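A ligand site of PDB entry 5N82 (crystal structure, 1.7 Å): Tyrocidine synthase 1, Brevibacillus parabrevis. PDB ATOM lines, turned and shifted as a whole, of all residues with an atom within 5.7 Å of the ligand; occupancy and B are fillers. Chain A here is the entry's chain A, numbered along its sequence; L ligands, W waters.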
ATOM      1  N   THR A 188       0.020  34.002  13.241  1.00  0.00           N
ATOM      2  CA  THR A 188      -0.436  32.980  12.313  1.00  0.00           C
ATOM      3  C   THR A 188      -1.840  32.549  12.689  1.00  0.00           C
ATOM      4  O   THR A 188      -2.301  32.805  13.811  1.00  0.00           O
ATOM      5  CB  THR A 188       0.479  31.748  12.312  1.00  0.00           C
ATOM      6  OG1 THR A 188       0.433  31.124  13.606  1.00  0.00           O
ATOM      7  CG2 THR A 188       1.910  32.139  11.971  1.00  0.00           C
ATOM      8  N   PHE A 232       5.327  37.001   6.856  1.00  0.00           N
ATOM      9  CA  PHE A 232       5.649  35.590   6.720  1.00  0.00           C
ATOM     10  C   PHE A 232       7.089  35.392   7.206  1.00  0.00           C
ATOM     11  O   PHE A 232       7.982  36.124   6.774  1.00  0.00           O
ATOM     12  CB  PHE A 232       5.496  35.183   5.256  1.00  0.00           C
ATOM     13  CG  PHE A 232       5.603  33.715   4.972  1.00  0.00           C
ATOM     14  CD1 PHE A 232       5.212  32.760   5.910  1.00  0.00           C
ATOM     15  CD2 PHE A 232       6.040  33.294   3.731  1.00  0.00           C
ATOM     16  CE1 PHE A 232       5.287  31.411   5.600  1.00  0.00           C
ATOM     17  CE2 PHE A 232       6.138  31.943   3.420  1.00  0.00           C
ATOM     18  CZ  PHE A 232       5.766  31.002   4.360  1.00  0.00           C
ATOM     19  N   ASP A 233       7.320  34.449   8.134  1.00  0.00           N
ATOM     20  CA  ASP A 233       8.653  34.451   8.728  1.00  0.00           C
ATOM     21  C   ASP A 233       9.753  34.022   7.759  1.00  0.00           C
ATOM     22  O   ASP A 233      10.932  34.152   8.105  1.00  0.00           O
ATOM     23  CB  ASP A 233       8.700  33.608  10.011  1.00  0.00           C
ATOM     24  CG  ASP A 233       8.647  32.111   9.781  1.00  0.00           C
ATOM     25  OD1 ASP A 233       8.440  31.675   8.626  1.00  0.00           O
ATOM     26  OD2 ASP A 233       8.829  31.367  10.777  1.00  0.00           O
ATOM     27  N   VAL A 234       9.430  33.561   6.546  1.00  0.00           N
ATOM     28  CA  VAL A 234      10.497  33.362   5.564  1.00  0.00           C
ATOM     29  C   VAL A 234      11.258  34.668   5.359  1.00  0.00           C
ATOM     30  O   VAL A 234      12.478  34.648   5.083  1.00  0.00           O
ATOM     31  CB  VAL A 234       9.925  32.824   4.241  1.00  0.00           C
ATOM     32  CG1 VAL A 234      11.006  32.798   3.172  1.00  0.00           C
ATOM     33  CG2 VAL A 234       9.338  31.423   4.434  1.00  0.00           C
ATOM     34  N   TRP A 237      14.224  34.884   7.729  1.00  0.00           N
ATOM     35  CA  TRP A 237      15.282  34.053   7.164  1.00  0.00           C
ATOM     36  C   TRP A 237      16.027  34.798   6.057  1.00  0.00           C
ATOM     37  O   TRP A 237      17.258  34.859   6.074  1.00  0.00           O
ATOM     38  CB  TRP A 237      14.637  32.748   6.693  1.00  0.00           C
ATOM     39  CG  TRP A 237      15.262  31.904   5.624  1.00  0.00           C
ATOM     40  CD1 TRP A 237      15.166  32.077   4.272  1.00  0.00           C
ATOM     41  CD2 TRP A 237      15.938  30.658   5.818  1.00  0.00           C
ATOM     42  NE1 TRP A 237      15.800  31.049   3.606  1.00  0.00           N
ATOM     43  CE2 TRP A 237      16.271  30.159   4.540  1.00  0.00           C
ATOM     44  CE3 TRP A 237      16.311  29.921   6.948  1.00  0.00           C
ATOM     45  CZ2 TRP A 237      16.986  28.963   4.354  1.00  0.00           C
ATOM     46  CZ3 TRP A 237      17.018  28.735   6.768  1.00  0.00           C
ATOM     47  CH2 TRP A 237      17.331  28.258   5.478  1.00  0.00           C
ATOM     48  N   THR A 298      13.811  26.289  -1.674  1.00  0.00           N
ATOM     49  CA  THR A 298      12.358  26.374  -1.576  1.00  0.00           C
ATOM     50  C   THR A 298      11.955  26.038  -0.152  1.00  0.00           C
ATOM     51  O   THR A 298      12.590  25.227   0.517  1.00  0.00           O
ATOM     52  CB  THR A 298      11.627  25.474  -2.583  1.00  0.00           C
ATOM     53  OG1 THR A 298      11.862  24.096  -2.293  1.00  0.00           O
ATOM     54  CG2 THR A 298      12.029  25.798  -4.024  1.00  0.00           C
ATOM     55  N   ALA A 299      10.891  26.701   0.308  1.00  0.00           N
ATOM     56  CA  ALA A 299      10.447  26.567   1.689  1.00  0.00           C
ATOM     57  C   ALA A 299       8.939  26.722   1.747  1.00  0.00           C
ATOM     58  O   ALA A 299       8.322  27.306   0.853  1.00  0.00           O
ATOM     59  CB  ALA A 299      11.103  27.616   2.584  1.00  0.00           C
ATOM     60  N   GLY A 300       8.353  26.184   2.827  1.00  0.00           N
ATOM     61  CA  GLY A 300       6.976  26.436   3.205  1.00  0.00           C
ATOM     62  C   GLY A 300       5.965  25.412   2.704  1.00  0.00           C
ATOM     63  O   GLY A 300       4.912  25.240   3.315  1.00  0.00           O
ATOM     64  N   SER A 301       6.260  24.756   1.589  1.00  0.00           N
ATOM     65  CA  SER A 301       5.337  23.798   0.990  1.00  0.00           C
ATOM     66  C   SER A 301       6.160  22.676   0.392  1.00  0.00           C
ATOM     67  O   SER A 301       7.349  22.828   0.104  1.00  0.00           O
ATOM     68  CB  SER A 301       4.462  24.472  -0.071  1.00  0.00           C
ATOM     69  OG  SER A 301       3.638  25.460   0.518  1.00  0.00           O
ATOM     70  N   ALA A 302       5.499  21.538   0.185  1.00  0.00           N
ATOM     71  CA  ALA A 302       6.195  20.369  -0.350  1.00  0.00           C
ATOM     72  C   ALA A 302       6.731  20.640  -1.744  1.00  0.00           C
ATOM     73  O   ALA A 302       6.020  21.150  -2.618  1.00  0.00           O
ATOM     74  CB  ALA A 302       5.251  19.175  -0.368  1.00  0.00           C
ATOM     75  N   SER A 303       7.995  20.289  -1.954  1.00  0.00           N
ATOM     76  CA  SER A 303       8.569  20.299  -3.291  1.00  0.00           C
ATOM     77  C   SER A 303       8.244  18.975  -3.977  1.00  0.00           C
ATOM     78  O   SER A 303       7.536  18.123  -3.436  1.00  0.00           O
ATOM     79  CB  SER A 303      10.078  20.545  -3.224  1.00  0.00           C
ATOM     80  OG  SER A 303      10.583  20.810  -4.516  1.00  0.00           O
ATOM     81  N   ASN A 319      15.945  22.234   0.065  1.00  0.00           N
ATOM     82  CA  ASN A 319      14.586  22.197   0.602  1.00  0.00           C
ATOM     83  C   ASN A 319      14.684  22.554   2.079  1.00  0.00           C
ATOM     84  O   ASN A 319      15.423  21.900   2.817  1.00  0.00           O
ATOM     85  CB  ASN A 319      13.970  20.807   0.409  1.00  0.00           C
ATOM     86  CG  ASN A 319      12.507  20.734   0.824  1.00  0.00           C
ATOM     87  OD1 ASN A 319      11.835  21.760   0.936  1.00  0.00           O
ATOM     88  ND2 ASN A 319      12.012  19.519   1.056  1.00  0.00           N
ATOM     89  N   ALA A 320      13.982  23.600   2.514  1.00  0.00           N
ATOM     90  CA  ALA A 320      14.068  24.055   3.893  1.00  0.00           C
ATOM     91  C   ALA A 320      12.704  23.963   4.549  1.00  0.00           C
ATOM     92  O   ALA A 320      11.724  24.496   4.014  1.00  0.00           O
ATOM     93  CB  ALA A 320      14.604  25.495   3.965  1.00  0.00           C
ATOM     94  N   TYR A 321      12.641  23.310   5.720  1.00  0.00           N
ATOM     95  CA  TYR A 321      11.393  23.044   6.418  1.00  0.00           C
ATOM     96  C   TYR A 321      11.404  23.627   7.817  1.00  0.00           C
ATOM     97  O   TYR A 321      12.401  23.557   8.543  1.00  0.00           O
ATOM     98  CB  TYR A 321      11.124  21.515   6.524  1.00  0.00           C
ATOM     99  CG  TYR A 321      10.214  21.139   7.694  1.00  0.00           C
ATOM    100  CD1 TYR A 321       8.839  21.089   7.539  1.00  0.00           C
ATOM    101  CD2 TYR A 321      10.750  20.845   8.956  1.00  0.00           C
ATOM    102  CE1 TYR A 321       7.992  20.758   8.615  1.00  0.00           C
ATOM    103  CE2 TYR A 321       9.922  20.523  10.025  1.00  0.00           C
ATOM    104  CZ  TYR A 321       8.557  20.482   9.852  1.00  0.00           C
ATOM    105  OH  TYR A 321       7.752  20.163  10.929  1.00  0.00           O
ATOM    106  N   GLY A 322      10.255  24.144   8.246  1.00  0.00           N
ATOM    107  CA  GLY A 322      10.079  24.436   9.643  1.00  0.00           C
ATOM    108  C   GLY A 322       8.707  25.019   9.905  1.00  0.00           C
ATOM    109  O   GLY A 322       8.046  25.539   8.996  1.00  0.00           O
ATOM    110  N   PRO A 323       8.250  24.940  11.145  1.00  0.00           N
ATOM    111  CA  PRO A 323       7.061  25.702  11.575  1.00  0.00           C
ATOM    112  C   PRO A 323       7.487  27.095  11.995  1.00  0.00           C
ATOM    113  O   PRO A 323       8.656  27.342  12.314  1.00  0.00           O
ATOM    114  CB  PRO A 323       6.563  24.900  12.781  1.00  0.00           C
ATOM    115  CG  PRO A 323       7.855  24.452  13.427  1.00  0.00           C
ATOM    116  CD  PRO A 323       8.811  24.156  12.266  1.00  0.00           C
ATOM    117  N   THR A 324       6.525  28.028  11.989  1.00  0.00           N
ATOM    118  CA  THR A 324       6.842  29.369  12.486  1.00  0.00           C
ATOM    119  C   THR A 324       7.397  29.313  13.904  1.00  0.00           C
ATOM    120  O   THR A 324       8.223  30.141  14.296  1.00  0.00           O
ATOM    121  CB  THR A 324       5.586  30.253  12.380  1.00  0.00           C
ATOM    122  OG1 THR A 324       5.304  30.453  10.990  1.00  0.00           O
ATOM    123  CG2 THR A 324       5.811  31.611  13.029  1.00  0.00           C
ATOM    124  N   GLU A 325       6.993  28.297  14.681  1.00  0.00           N
ATOM    125  CA  GLU A 325       7.382  28.205  16.075  1.00  0.00           C
ATOM    126  C   GLU A 325       8.866  27.898  16.307  1.00  0.00           C
ATOM    127  O   GLU A 325       9.318  27.903  17.456  1.00  0.00           O
ATOM    128  CB  GLU A 325       6.487  27.151  16.761  1.00  0.00           C
ATOM    129  CG  GLU A 325       5.018  27.564  16.984  1.00  0.00           C
ATOM    130  CD  GLU A 325       4.088  27.350  15.780  1.00  0.00           C
ATOM    131  OE1 GLU A 325       4.570  26.995  14.684  1.00  0.00           O
ATOM    132  OE2 GLU A 325       2.851  27.546  15.921  1.00  0.00           O
ATOM    133  N   LEU A 327      11.034  28.963  13.335  1.00  0.00           N
ATOM    134  CA  LEU A 327      11.449  29.514  12.047  1.00  0.00           C
ATOM    135  C   LEU A 327      11.782  28.385  11.076  1.00  0.00           C
ATOM    136  O   LEU A 327      11.030  28.132  10.132  1.00  0.00           O
ATOM    137  CB  LEU A 327      12.642  30.466  12.211  1.00  0.00           C
ATOM    138  CG  LEU A 327      13.151  31.090  10.903  1.00  0.00           C
ATOM    139  CD1 LEU A 327      12.046  31.883  10.236  1.00  0.00           C
ATOM    140  CD2 LEU A 327      14.394  31.962  11.150  1.00  0.00           C
ATOM    141  N   VAL A 328      12.891  27.699  11.306  1.00  0.00           N
ATOM    142  CA  VAL A 328      13.372  26.645  10.417  1.00  0.00           C
ATOM    143  C   VAL A 328      13.946  25.519  11.268  1.00  0.00           C
ATOM    144  O   VAL A 328      14.609  25.771  12.279  1.00  0.00           O
ATOM    145  CB  VAL A 328      14.418  27.177   9.411  1.00  0.00           C
ATOM    146  CG1 VAL A 328      15.604  27.748  10.152  1.00  0.00           C
ATOM    147  CG2 VAL A 328      14.879  26.072   8.450  1.00  0.00           C
ATOM    148  N   ILE A 346      12.802  16.335   3.620  1.00  0.00           N
ATOM    149  CA  ILE A 346      13.076  17.638   4.241  1.00  0.00           C
ATOM    150  C   ILE A 346      14.436  17.635   4.941  1.00  0.00           C
ATOM    151  O   ILE A 346      14.876  18.712   5.396  1.00  0.00           O
ATOM    152  CB  ILE A 346      11.965  18.088   5.208  1.00  0.00           C
ATOM    153  CG1 ILE A 346      11.649  17.002   6.247  1.00  0.00           C
ATOM    154  CG2 ILE A 346      10.683  18.483   4.417  1.00  0.00           C
ATOM    155  CD1 ILE A 346      10.694  17.468   7.323  1.00  0.00           C
ATOM    156  N   THR A 409       4.744  19.682  16.377  1.00  0.00           N
ATOM    157  CA  THR A 409       4.393  20.416  15.164  1.00  0.00           C
ATOM    158  C   THR A 409       3.029  20.057  14.599  1.00  0.00           C
ATOM    159  O   THR A 409       2.460  20.861  13.847  1.00  0.00           O
ATOM    160  CB  THR A 409       5.410  20.185  14.041  1.00  0.00           C
ATOM    161  OG1 THR A 409       5.356  18.812  13.637  1.00  0.00           O
ATOM    162  CG2 THR A 409       6.844  20.576  14.460  1.00  0.00           C
ATOM    163  N   ASP A 411       2.946  17.892  12.314  1.00  0.00           N
ATOM    164  CA  ASP A 411       3.363  17.335  11.042  1.00  0.00           C
ATOM    165  C   ASP A 411       3.698  15.859  11.197  1.00  0.00           C
ATOM    166  O   ASP A 411       4.294  15.434  12.193  1.00  0.00           O
ATOM    167  CB  ASP A 411       4.592  18.062  10.491  1.00  0.00           C
ATOM    168  CG  ASP A 411       4.305  19.503  10.094  1.00  0.00           C
ATOM    169  OD1 ASP A 411       3.205  19.774   9.546  1.00  0.00           O
ATOM    170  OD2 ASP A 411       5.191  20.366  10.292  1.00  0.00           O
ATOM    171  N   PHE A 423       8.936  14.179   4.950  1.00  0.00           N
ATOM    172  CA  PHE A 423       7.721  14.874   5.377  1.00  0.00           C
ATOM    173  C   PHE A 423       6.490  14.217   4.754  1.00  0.00           C
ATOM    174  O   PHE A 423       6.475  13.936   3.556  1.00  0.00           O
ATOM    175  CB  PHE A 423       7.807  16.349   4.976  1.00  0.00           C
ATOM    176  CG  PHE A 423       6.582  17.155   5.285  1.00  0.00           C
ATOM    177  CD1 PHE A 423       5.652  17.447   4.294  1.00  0.00           C
ATOM    178  CD2 PHE A 423       6.376  17.668   6.556  1.00  0.00           C
ATOM    179  CE1 PHE A 423       4.530  18.213   4.573  1.00  0.00           C
ATOM    180  CE2 PHE A 423       5.249  18.432   6.849  1.00  0.00           C
ATOM    181  CZ  PHE A 423       4.316  18.694   5.853  1.00  0.00           C
ATOM    182  N   GLY A 425       3.003  15.295   5.441  1.00  0.00           N
ATOM    183  CA  GLY A 425       1.783  16.032   5.675  1.00  0.00           C
ATOM    184  C   GLY A 425       1.476  16.228   7.144  1.00  0.00           C
ATOM    185  O   GLY A 425       2.387  16.462   7.944  1.00  0.00           O
ATOM    186  N   ARG A 426       0.199  16.127   7.514  1.00  0.00           N
ATOM    187  CA  ARG A 426      -0.264  16.432   8.867  1.00  0.00           C
ATOM    188  C   ARG A 426      -0.720  15.156   9.563  1.00  0.00           C
ATOM    189  O   ARG A 426      -1.273  14.251   8.925  1.00  0.00           O
ATOM    190  CB  ARG A 426      -1.424  17.441   8.839  1.00  0.00           C
ATOM    191  CG  ARG A 426      -1.087  18.773   8.176  1.00  0.00           C
ATOM    192  CD  ARG A 426      -0.125  19.621   9.008  1.00  0.00           C
ATOM    193  NE  ARG A 426      -0.748  20.103  10.237  1.00  0.00           N
ATOM    194  CZ  ARG A 426      -0.099  20.637  11.270  1.00  0.00           C
ATOM    195  NH1 ARG A 426       1.219  20.791  11.244  1.00  0.00           N
ATOM    196  NH2 ARG A 426      -0.779  21.028  12.348  1.00  0.00           N
HETATM  197  C1  LIG L   1       6.589  22.396   4.674  1.00  0.00           C
HETATM  198  C2  LIG L   1       7.844  22.777   4.354  1.00  0.00           C
HETATM  199  C3  LIG L   1       8.546  22.085   3.443  1.00  0.00           C
HETATM  200  C4  LIG L   1       7.038  24.137   5.845  1.00  0.00           C
HETATM  201  N1  LIG L   1       8.027  21.002   2.832  1.00  0.00           N
HETATM  202  N2  LIG L   1       6.017  21.320   4.099  1.00  0.00           N
HETATM  203  C5  LIG L   1      10.854  29.641   7.162  1.00  0.00           C
HETATM  204  C6  LIG L   1      12.165  29.772   6.687  1.00  0.00           C
HETATM  205  C7  LIG L   1      12.843  28.676   6.155  1.00  0.00           C
HETATM  206  C8  LIG L   1      12.195  27.442   6.091  1.00  0.00           C
HETATM  207  C9  LIG L   1      10.877  27.329   6.543  1.00  0.00           C
HETATM  208  C10 LIG L   1      10.192  28.405   7.100  1.00  0.00           C
HETATM  209  C11 LIG L   1       8.859  28.243   7.549  1.00  0.00           C
HETATM  210  N3  LIG L   1       8.587  28.884   8.850  1.00  0.00           N
HETATM  211  C12 LIG L   1       7.876  28.751   6.460  1.00  0.00           C
HETATM  212  C13 LIG L   1       6.412  28.353   6.736  1.00  0.00           C
HETATM  213  O1  LIG L   1       5.722  27.891   5.826  1.00  0.00           O
HETATM  214  N4  LIG L   1       5.967  28.587   7.967  1.00  0.00           N
HETATM  215  S1  LIG L   1       4.353  28.293   8.272  1.00  0.00           S
HETATM  216  O2  LIG L   1       4.109  28.527   9.759  1.00  0.00           O
HETATM  217  O3  LIG L   1       3.481  29.176   7.410  1.00  0.00           O
HETATM  218  O4  LIG L   1       3.982  26.858   7.910  1.00  0.00           O
HETATM  219  C14 LIG L   1       4.648  25.773   8.549  1.00  0.00           C
HETATM  220  C15 LIG L   1       4.186  24.460   7.998  1.00  0.00           C
HETATM  221  O5  LIG L   1       4.360  24.404   6.568  1.00  0.00           O
HETATM  222  C16 LIG L   1       4.944  23.239   8.501  1.00  0.00           C
HETATM  223  O6  LIG L   1       4.537  22.841   9.811  1.00  0.00           O
HETATM  224  C17 LIG L   1       4.662  22.219   7.415  1.00  0.00           C
HETATM  225  O7  LIG L   1       3.333  21.712   7.537  1.00  0.00           O
HETATM  226  C18 LIG L   1       4.747  23.108   6.175  1.00  0.00           C
HETATM  227  N5  LIG L   1       6.108  23.213   5.594  1.00  0.00           N
HETATM  228  N6  LIG L   1       8.108  23.865   5.088  1.00  0.00           N
HETATM  229  C19 LIG L   1       6.733  20.592   3.150  1.00  0.00           C
HETATM  230  N7  LIG L   1       9.791  22.458   3.140  1.00  0.00           N
HETATM  231  O   HOH W   1       2.793  24.346  11.238  1.00  0.00           O
HETATM  232  O   HOH W   2       9.143  19.355   0.833  1.00  0.00           O
HETATM  233  O   HOH W   3       1.146  30.109   9.393  1.00  0.00           O
HETATM  234  O   HOH W   4       3.755  26.952  12.126  1.00  0.00           O
HETATM  235  O   HOH W   5       3.327  26.832   4.935  1.00  0.00           O
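O of Ala 320 is in hydrogen-bond range of N7 of the ligand, 2.9 Å away.
The side-chain carboxylate (OD1) of Asp 233 lies within salt-bridge range of a nitrogen (N3) of the ligand (2.8 Å).
A nitrogen (N3) of the ligand is in hydrogen-bond range of the backbone carbonyl oxygen of Leu 327 (2.9 Å).
OG1 of Thr 324 lies within hydrogen-bond range of O2 of the ligand (2.6 Å).
A nitrogen (N3) of the ligand lies close to the backbone carbonyl oxygen (O) of Gly 322, 3.4 Å away.
OD1 of Asn 319 lies within hydrogen-bond range of N7 of the ligand (3.1 Å).
An oxygen (O2) of the ligand is in hydrogen-bond range of the backbone NH (N) of Thr 324, at 3.3 Å.
A nitrogen (N6) of the ligand sits at hydrogen-bond distance from the backbone NH of Gly 300, at 3.2 Å.
O6 of the ligand sits at hydrogen-bond distance from OD2 of Asp 411 (2.6 Å).
The backbone NH of Ala 320 lies within hydrogen-bond range of the backbone carbonyl oxygen of Thr 298 (2.9 Å).
OH of Tyr 321 lies within hydrogen-bond range of OD2 of Asp 411 (2.6 Å).
OD1 of Asp 411 lies within salt-bridge range of NH1 of Arg 426 (2.8 Å).
The side-chain hydroxyl (OG1) of Thr 409 lies within hydrogen-bond range of the backbone NH (N) of Asp 411.
O of Ser 301 sits close to N1 of the ligand (3.4 Å).
Phe 232 touches the ligand.
CG2 of Val 234 touches C5 of the ligand (3.6 Å).
CD2 of Trp 237 touches C7 of the ligand, at 3.7 Å.
CB of Ala 299 touches C8 of the ligand, at 3.7 Å.
Ala 302 touches the ligand.
Tyr 321 touches the ligand (CA to N6, 3.6 Å).
Pro 323 touches the ligand.
Val 328 touches the ligand.
CG2 of Ile 346 touches N1 of the ligand (3.99 Å).
CE1 of Phe 423 touches N2 of the ligand, at 3.5 Å.
Hydrophobic or aromatic side chains that line the ligand: Phe 232, Val 234, Trp 237, Ala 299, Ala 320, Tyr 321, Leu 327, Val 328, Ile 346 and Phe 423.
Of the 26 residues printed, 19 come within 4 Å of the ligand.
The nearest printed residue that does not touch the ligand is Arg 426 (4.2 Å).
Water W5 lies within hydrogen-bond range of O1 of the ligand (2.8 Å) and O of Gly 300 (2.8 Å).
Water W2 lies within hydrogen-bond range of N1 of the ligand (2.8 Å), ND2 of Asn 319 (2.9 Å) and N of Ser 303 (3.2 Å).
Water W4 lies within hydrogen-bond range of OE1 of Glu 325 (2.7 Å), O2 of the ligand (2.9 Å) and N of Thr 324 (3.0 Å).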
